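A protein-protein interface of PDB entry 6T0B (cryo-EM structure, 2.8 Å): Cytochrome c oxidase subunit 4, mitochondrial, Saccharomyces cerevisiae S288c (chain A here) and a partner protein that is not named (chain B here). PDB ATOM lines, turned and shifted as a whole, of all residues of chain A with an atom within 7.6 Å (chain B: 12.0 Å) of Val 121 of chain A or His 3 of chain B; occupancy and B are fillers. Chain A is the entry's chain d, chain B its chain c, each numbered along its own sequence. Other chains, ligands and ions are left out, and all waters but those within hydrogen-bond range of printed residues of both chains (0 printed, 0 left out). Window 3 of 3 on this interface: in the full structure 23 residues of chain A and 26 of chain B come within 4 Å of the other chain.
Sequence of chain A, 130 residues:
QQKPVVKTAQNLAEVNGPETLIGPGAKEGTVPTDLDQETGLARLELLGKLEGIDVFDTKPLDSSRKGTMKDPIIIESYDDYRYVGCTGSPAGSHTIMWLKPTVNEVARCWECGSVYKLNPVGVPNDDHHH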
ATOM      1  N   ILE A  75      11.649 -21.987  12.436  1.00  0.00           N
ATOM      2  CA  ILE A  75      11.864 -22.374  13.822  1.00  0.00           C
ATOM      3  C   ILE A  75      12.004 -21.102  14.645  1.00  0.00           C
ATOM      4  O   ILE A  75      12.854 -20.255  14.355  1.00  0.00           O
ATOM      5  CB  ILE A  75      13.104 -23.263  13.969  1.00  0.00           C
ATOM      6  CG1 ILE A  75      13.121 -24.340  12.899  1.00  0.00           C
ATOM      7  CG2 ILE A  75      13.142 -23.906  15.314  1.00  0.00           C
ATOM      8  CD1 ILE A  75      11.990 -25.316  12.993  1.00  0.00           C
ATOM      9  N   GLU A  76      11.167 -20.966  15.662  1.00  0.00           N
ATOM     10  CA  GLU A  76      11.182 -19.806  16.534  1.00  0.00           C
ATOM     11  C   GLU A  76      12.246 -19.999  17.594  1.00  0.00           C
ATOM     12  O   GLU A  76      12.335 -21.075  18.187  1.00  0.00           O
ATOM     13  CB  GLU A  76       9.816 -19.623  17.188  1.00  0.00           C
ATOM     14  CG  GLU A  76       8.666 -19.417  16.211  1.00  0.00           C
ATOM     15  CD  GLU A  76       8.006 -20.716  15.761  1.00  0.00           C
ATOM     16  OE1 GLU A  76       8.610 -21.798  15.934  1.00  0.00           O
ATOM     17  OE2 GLU A  76       6.880 -20.654  15.227  1.00  0.00           O
ATOM     18  N   SER A  77      13.050 -18.971  17.844  1.00  0.00           N
ATOM     19  CA  SER A  77      14.070 -19.112  18.871  1.00  0.00           C
ATOM     20  C   SER A  77      14.254 -17.821  19.644  1.00  0.00           C
ATOM     21  O   SER A  77      14.077 -16.729  19.115  1.00  0.00           O
ATOM     22  CB  SER A  77      15.413 -19.523  18.299  1.00  0.00           C
ATOM     23  OG  SER A  77      16.441 -19.220  19.219  1.00  0.00           O
ATOM     24  N   TYR A  78      14.625 -17.968  20.908  1.00  0.00           N
ATOM     25  CA  TYR A  78      14.870 -16.844  21.791  1.00  0.00           C
ATOM     26  C   TYR A  78      16.337 -16.469  21.854  1.00  0.00           C
ATOM     27  O   TYR A  78      16.725 -15.656  22.695  1.00  0.00           O
ATOM     28  CB  TYR A  78      14.341 -17.155  23.185  1.00  0.00           C
ATOM     29  CG  TYR A  78      12.857 -16.979  23.294  1.00  0.00           C
ATOM     30  CD1 TYR A  78      12.311 -15.743  23.551  1.00  0.00           C
ATOM     31  CD2 TYR A  78      12.002 -18.043  23.122  1.00  0.00           C
ATOM     32  CE1 TYR A  78      10.959 -15.570  23.639  1.00  0.00           C
ATOM     33  CE2 TYR A  78      10.645 -17.880  23.208  1.00  0.00           C
ATOM     34  CZ  TYR A  78      10.132 -16.641  23.466  1.00  0.00           C
ATOM     35  OH  TYR A  78       8.779 -16.474  23.559  1.00  0.00           O
ATOM     36  N   ASP A  79      17.161 -17.047  20.989  1.00  0.00           N
ATOM     37  CA  ASP A  79      18.537 -16.623  20.807  1.00  0.00           C
ATOM     38  C   ASP A  79      18.838 -16.698  19.320  1.00  0.00           C
ATOM     39  O   ASP A  79      17.935 -16.846  18.495  1.00  0.00           O
ATOM     40  CB  ASP A  79      19.488 -17.476  21.649  1.00  0.00           C
ATOM     41  CG  ASP A  79      19.123 -18.920  21.624  1.00  0.00           C
ATOM     42  OD1 ASP A  79      18.166 -19.261  20.908  1.00  0.00           O
ATOM     43  OD2 ASP A  79      19.777 -19.720  22.321  1.00  0.00           O
ATOM     44  N   ARG A  82      19.450 -22.375  16.951  1.00  0.00           N
ATOM     45  CA  ARG A  82      18.694 -23.449  17.590  1.00  0.00           C
ATOM     46  C   ARG A  82      19.076 -24.787  16.994  1.00  0.00           C
ATOM     47  O   ARG A  82      19.075 -24.937  15.777  1.00  0.00           O
ATOM     48  CB  ARG A  82      17.195 -23.253  17.432  1.00  0.00           C
ATOM     49  CG  ARG A  82      16.400 -24.267  18.191  1.00  0.00           C
ATOM     50  CD  ARG A  82      15.057 -23.741  18.532  1.00  0.00           C
ATOM     51  NE  ARG A  82      14.283 -24.733  19.244  1.00  0.00           N
ATOM     52  CZ  ARG A  82      13.116 -24.481  19.798  1.00  0.00           C
ATOM     53  NH1 ARG A  82      12.606 -23.269  19.721  1.00  0.00           N
ATOM     54  NH2 ARG A  82      12.467 -25.434  20.435  1.00  0.00           N
ATOM     55  N   LEU A 118      15.445 -19.695  10.778  1.00  0.00           N
ATOM     56  CA  LEU A 118      15.240 -19.337  12.167  1.00  0.00           C
ATOM     57  C   LEU A 118      14.671 -17.935  12.239  1.00  0.00           C
ATOM     58  O   LEU A 118      15.183 -17.029  11.580  1.00  0.00           O
ATOM     59  CB  LEU A 118      16.558 -19.382  12.923  1.00  0.00           C
ATOM     60  CG  LEU A 118      16.429 -19.372  14.423  1.00  0.00           C
ATOM     61  CD1 LEU A 118      16.218 -20.780  14.871  1.00  0.00           C
ATOM     62  CD2 LEU A 118      17.677 -18.806  15.000  1.00  0.00           C
ATOM     63  N   ASN A 119      13.622 -17.747  13.032  1.00  0.00           N
ATOM     64  CA  ASN A 119      13.299 -16.368  13.345  1.00  0.00           C
ATOM     65  C   ASN A 119      13.526 -16.105  14.821  1.00  0.00           C
ATOM     66  O   ASN A 119      13.098 -16.895  15.677  1.00  0.00           O
ATOM     67  CB  ASN A 119      11.872 -15.989  12.950  1.00  0.00           C
ATOM     68  CG  ASN A 119      10.845 -16.793  13.647  1.00  0.00           C
ATOM     69  OD1 ASN A 119      10.985 -18.001  13.790  1.00  0.00           O
ATOM     70  ND2 ASN A 119       9.797 -16.135  14.108  1.00  0.00           N
ATOM     71  N   PRO A 120      14.279 -15.067  15.142  1.00  0.00           N
ATOM     72  CA  PRO A 120      14.550 -14.739  16.542  1.00  0.00           C
ATOM     73  C   PRO A 120      13.427 -13.909  17.143  1.00  0.00           C
ATOM     74  O   PRO A 120      13.230 -12.746  16.787  1.00  0.00           O
ATOM     75  CB  PRO A 120      15.867 -13.962  16.464  1.00  0.00           C
ATOM     76  CG  PRO A 120      15.919 -13.437  15.105  1.00  0.00           C
ATOM     77  CD  PRO A 120      15.178 -14.356  14.225  1.00  0.00           C
ATOM     78  N   VAL A 121      12.693 -14.511  18.076  1.00  0.00           N
ATOM     79  CA  VAL A 121      11.606 -13.810  18.741  1.00  0.00           C
ATOM     80  C   VAL A 121      12.054 -13.139  20.022  1.00  0.00           C
ATOM     81  O   VAL A 121      11.316 -12.304  20.563  1.00  0.00           O
ATOM     82  CB  VAL A 121      10.449 -14.772  19.046  1.00  0.00           C
ATOM     83  CG1 VAL A 121       9.887 -15.330  17.763  1.00  0.00           C
ATOM     84  CG2 VAL A 121      10.925 -15.886  19.936  1.00  0.00           C
ATOM     85  N   GLY A 122      13.235 -13.466  20.525  1.00  0.00           N
ATOM     86  CA  GLY A 122      13.717 -12.898  21.761  1.00  0.00           C
ATOM     87  C   GLY A 122      14.290 -11.512  21.570  1.00  0.00           C
ATOM     88  O   GLY A 122      14.207 -10.902  20.503  1.00  0.00           O
ATOM     89  N   VAL A 123      14.873 -11.002  22.647  1.00  0.00           N
ATOM     90  CA  VAL A 123      15.560  -9.719  22.597  1.00  0.00           C
ATOM     91  C   VAL A 123      17.040  -9.958  22.871  1.00  0.00           C
ATOM     92  O   VAL A 123      17.394 -10.857  23.648  1.00  0.00           O
ATOM     93  CB  VAL A 123      14.935  -8.710  23.573  1.00  0.00           C
ATOM     94  CG1 VAL A 123      13.508  -8.430  23.170  1.00  0.00           C
ATOM     95  CG2 VAL A 123      14.971  -9.221  24.995  1.00  0.00           C
ATOM     96  N   PRO A 124      17.940  -9.236  22.201  1.00  0.00           N
ATOM     97  CA  PRO A 124      19.368  -9.371  22.480  1.00  0.00           C
ATOM     98  C   PRO A 124      19.872  -8.291  23.435  1.00  0.00           C
ATOM     99  O   PRO A 124      19.063  -7.717  24.167  1.00  0.00           O
ATOM    100  CB  PRO A 124      19.994  -9.225  21.099  1.00  0.00           C
ATOM    101  CG  PRO A 124      19.082  -8.274  20.398  1.00  0.00           C
ATOM    102  CD  PRO A 124      17.696  -8.476  20.965  1.00  0.00           C
ATOM    103  N   MET B   1       1.468 -13.590  27.415  1.00  0.00           N
ATOM    104  CA  MET B   1       2.485 -12.581  27.674  1.00  0.00           C
ATOM    105  C   MET B   1       3.335 -12.334  26.423  1.00  0.00           C
ATOM    106  O   MET B   1       3.410 -13.184  25.539  1.00  0.00           O
ATOM    107  CB  MET B   1       3.358 -13.003  28.865  1.00  0.00           C
ATOM    108  CG  MET B   1       4.274 -14.180  28.598  1.00  0.00           C
ATOM    109  SD  MET B   1       5.525 -14.521  29.829  1.00  0.00           S
ATOM    110  CE  MET B   1       4.925 -15.826  30.700  1.00  0.00           C
ATOM    111  N   THR B   2       3.953 -11.159  26.341  1.00  0.00           N
ATOM    112  CA  THR B   2       4.669 -10.779  25.137  1.00  0.00           C
ATOM    113  C   THR B   2       6.018 -11.478  25.065  1.00  0.00           C
ATOM    114  O   THR B   2       6.486 -12.083  26.026  1.00  0.00           O
ATOM    115  CB  THR B   2       4.873  -9.273  25.073  1.00  0.00           C
ATOM    116  OG1 THR B   2       5.915  -8.895  25.971  1.00  0.00           O
ATOM    117  CG2 THR B   2       3.612  -8.561  25.454  1.00  0.00           C
ATOM    118  N   HIS B   3       6.640 -11.383  23.889  1.00  0.00           N
ATOM    119  CA  HIS B   3       7.961 -11.961  23.680  1.00  0.00           C
ATOM    120  C   HIS B   3       9.010 -11.247  24.516  1.00  0.00           C
ATOM    121  O   HIS B   3       9.928 -11.885  25.055  1.00  0.00           O
ATOM    122  CB  HIS B   3       8.323 -11.879  22.202  1.00  0.00           C
ATOM    123  CG  HIS B   3       7.754 -12.986  21.374  1.00  0.00           C
ATOM    124  ND1 HIS B   3       7.908 -14.314  21.702  1.00  0.00           N
ATOM    125  CD2 HIS B   3       7.047 -12.965  20.223  1.00  0.00           C
ATOM    126  CE1 HIS B   3       7.323 -15.062  20.787  1.00  0.00           C
ATOM    127  NE2 HIS B   3       6.790 -14.268  19.879  1.00  0.00           N
ATOM    128  N   LEU B   4       8.865  -9.926  24.649  1.00  0.00           N
ATOM    129  CA  LEU B   4       9.814  -9.109  25.392  1.00  0.00           C
ATOM    130  C   LEU B   4       9.847  -9.495  26.858  1.00  0.00           C
ATOM    131  O   LEU B   4      10.905  -9.479  27.494  1.00  0.00           O
ATOM    132  CB  LEU B   4       9.438  -7.640  25.240  1.00  0.00           C
ATOM    133  CG  LEU B   4      10.111  -6.623  26.145  1.00  0.00           C
ATOM    134  CD1 LEU B   4      11.533  -6.383  25.691  1.00  0.00           C
ATOM    135  CD2 LEU B   4       9.316  -5.343  26.152  1.00  0.00           C
ATOM    136  N   GLU B   5       8.708  -9.886  27.397  1.00  0.00           N
ATOM    137  CA  GLU B   5       8.635 -10.230  28.799  1.00  0.00           C
ATOM    138  C   GLU B   5       8.841 -11.715  29.043  1.00  0.00           C
ATOM    139  O   GLU B   5       9.335 -12.091  30.108  1.00  0.00           O
ATOM    140  CB  GLU B   5       7.299  -9.745  29.357  1.00  0.00           C
ATOM    141  CG  GLU B   5       7.223  -9.759  30.821  1.00  0.00           C
ATOM    142  CD  GLU B   5       6.592 -10.994  31.327  1.00  0.00           C
ATOM    143  OE1 GLU B   5       5.651 -11.456  30.669  1.00  0.00           O
ATOM    144  OE2 GLU B   5       7.076 -11.541  32.344  1.00  0.00           O
ATOM    145  N   ARG B   6       8.475 -12.568  28.088  1.00  0.00           N
ATOM    146  CA  ARG B   6       8.808 -13.986  28.172  1.00  0.00           C
ATOM    147  C   ARG B   6      10.307 -14.202  28.103  1.00  0.00           C
ATOM    148  O   ARG B   6      10.820 -15.171  28.666  1.00  0.00           O
ATOM    149  CB  ARG B   6       8.115 -14.752  27.049  1.00  0.00           C
ATOM    150  CG  ARG B   6       8.293 -16.261  27.054  1.00  0.00           C
ATOM    151  CD  ARG B   6       7.933 -16.846  28.396  1.00  0.00           C
ATOM    152  NE  ARG B   6       8.139 -18.284  28.492  1.00  0.00           N
ATOM    153  CZ  ARG B   6       9.127 -18.850  29.165  1.00  0.00           C
ATOM    154  NH1 ARG B   6       9.217 -20.159  29.200  1.00  0.00           N
ATOM    155  NH2 ARG B   6      10.020 -18.111  29.799  1.00  0.00           N
ATOM    156  N   SER B   7      11.032 -13.297  27.453  1.00  0.00           N
ATOM    157  CA  SER B   7      12.474 -13.446  27.369  1.00  0.00           C
ATOM    158  C   SER B   7      13.190 -13.178  28.685  1.00  0.00           C
ATOM    159  O   SER B   7      14.388 -13.452  28.773  1.00  0.00           O
ATOM    160  CB  SER B   7      13.013 -12.523  26.285  1.00  0.00           C
ATOM    161  OG  SER B   7      12.282 -12.694  25.090  1.00  0.00           O
ATOM    162  N   ARG B   8      12.507 -12.664  29.706  1.00  0.00           N
ATOM    163  CA  ARG B   8      13.122 -12.439  31.006  1.00  0.00           C
ATOM    164  C   ARG B   8      12.929 -13.598  31.968  1.00  0.00           C
ATOM    165  O   ARG B   8      12.912 -13.379  33.180  1.00  0.00           O
ATOM    166  CB  ARG B   8      12.574 -11.171  31.646  1.00  0.00           C
ATOM    167  CG  ARG B   8      12.525  -9.994  30.739  1.00  0.00           C
ATOM    168  CD  ARG B   8      11.505  -9.011  31.243  1.00  0.00           C
ATOM    169  NE  ARG B   8      11.966  -8.320  32.437  1.00  0.00           N
ATOM    170  CZ  ARG B   8      11.214  -7.491  33.147  1.00  0.00           C
ATOM    171  NH1 ARG B   8       9.963  -7.256  32.785  1.00  0.00           N
ATOM    172  NH2 ARG B   8      11.712  -6.901  34.221  1.00  0.00           N
ATOM    173  N   HIS B   9      12.755 -14.814  31.467  1.00  0.00           N
ATOM    174  CA  HIS B   9      12.598 -15.986  32.311  1.00  0.00           C
ATOM    175  C   HIS B   9      13.359 -17.126  31.654  1.00  0.00           C
ATOM    176  O   HIS B   9      14.136 -16.916  30.721  1.00  0.00           O
ATOM    177  CB  HIS B   9      11.118 -16.300  32.535  1.00  0.00           C
ATOM    178  CG  HIS B   9      10.382 -15.244  33.299  1.00  0.00           C
ATOM    179  ND1 HIS B   9       9.863 -14.119  32.704  1.00  0.00           N
ATOM    180  CD2 HIS B   9      10.063 -15.152  34.609  1.00  0.00           C
ATOM    181  CE1 HIS B   9       9.257 -13.379  33.611  1.00  0.00           C
ATOM    182  NE2 HIS B   9       9.369 -13.981  34.776  1.00  0.00           N
ATOM    183  N   GLN B  10      13.132 -18.350  32.112  1.00  0.00           N
ATOM    184  CA  GLN B  10      14.155 -19.369  31.930  1.00  0.00           C
ATOM    185  C   GLN B  10      14.015 -20.218  30.674  1.00  0.00           C
ATOM    186  O   GLN B  10      14.996 -20.870  30.301  1.00  0.00           O
ATOM    187  CB  GLN B  10      14.198 -20.298  33.142  1.00  0.00           C
ATOM    188  CG  GLN B  10      15.606 -20.662  33.519  1.00  0.00           C
ATOM    189  CD  GLN B  10      15.677 -21.657  34.623  1.00  0.00           C
ATOM    190  OE1 GLN B  10      14.762 -21.774  35.417  1.00  0.00           O
ATOM    191  NE2 GLN B  10      16.772 -22.384  34.690  1.00  0.00           N
ATOM    192  N   GLN B  11      12.834 -20.276  30.054  1.00  0.00           N
ATOM    193  CA  GLN B  11      12.473 -21.058  28.862  1.00  0.00           C
ATOM    194  C   GLN B  11      12.465 -22.568  29.079  1.00  0.00           C
ATOM    195  O   GLN B  11      12.071 -23.293  28.165  1.00  0.00           O
ATOM    196  CB  GLN B  11      13.361 -20.784  27.635  1.00  0.00           C
ATOM    197  CG  GLN B  11      13.305 -19.384  27.091  1.00  0.00           C
ATOM    198  CD  GLN B  11      11.997 -19.086  26.426  1.00  0.00           C
ATOM    199  OE1 GLN B  11      11.465 -17.984  26.546  1.00  0.00           O
ATOM    200  NE2 GLN B  11      11.456 -20.069  25.722  1.00  0.00           N
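Of the 13 printed residues of chain A, 4 touch a printed residue of chain B. Printed residues of chain A that touch a printed residue of chain B: Tyr 78, Val 121, Gly 122 and Val 123. Hydrophobic or aromatic side chains of chain A that line the printed part of chain B: Tyr 78, Val 121 and Val 123. Among the printed residues, 8 pairs touch across the chains. Among the printed residues, no Asp or Glu carboxylate lies within 4 Å of a Lys or Arg side-chain nitrogen of the other chain.
Val 121 of chain A touches one residue of chain B. Printed residues of chain A within 4 Å of His 3 of chain B: Tyr 78 (3.0 Å) and Val 121 (3.4 Å). No residue of chain B comes within 4 Å of Glu 76 of chain A. No residue of chain B comes within 4 Å of Ser 77 of chain A. Of chain B, only His 3, Arg 6, Ser 7 and Gln 11 come within 4 Å of Tyr 78 of chain A. No residue of chain B comes within 4 Å of Asn 119 of chain A. No residue of chain B comes within 4 Å of Pro 120 of chain A. Of chain B, only Ser 7 (3.6 Å) comes within 4 Å of Gly 122 of chain A. Printed residues of chain A within 4 Å of Arg 6 of chain B: Tyr 78 (3.5 Å). Of the printed residues of chain A, Ser 7 of chain B touches Tyr 78, Gly 122 and Val 123. Of the printed residues of chain A, Leu 4 of chain B touches Val 123. Of the printed residues of chain A, Gln 11 of chain B touches Tyr 78. Gln 10 of chain B touches none of the printed residues of chain A.
ND1 of His 3 of chain B sits at hydrogen-bond distance from OH of Tyr 78 of chain A.
The side-chain hydroxyl (OG1) of Thr 2 of chain B sits close to the backbone NH (N) of Leu 4 of chain B. The backbone carbonyl oxygen (O) of Ser 77 of chain A is in hydrogen-bond range of the backbone NH (N) of Val 121 of chain A (2.8 Å). OG of Ser 7 of chain B is in hydrogen-bond range of O of His 3 of chain B (2.5 Å).
Among the printed residues, merely in contact across the chains: Tyr 78 of chain A with Gln 11 of chain B (3.3 Å), Tyr 78 of chain A with Ser 7 of chain B (3.4 Å), Val 121 of chain A with His 3 of chain B (3.4 Å), Tyr 78 of chain A with Arg 6 of chain B (3.5 Å), Gly 122 of chain A with Ser 7 of chain B (3.6 Å), Val 123 of chain A with Leu 4 of chain B (3.8 Å) and Val 123 of chain A with Ser 7 of chain B (3.9 Å).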
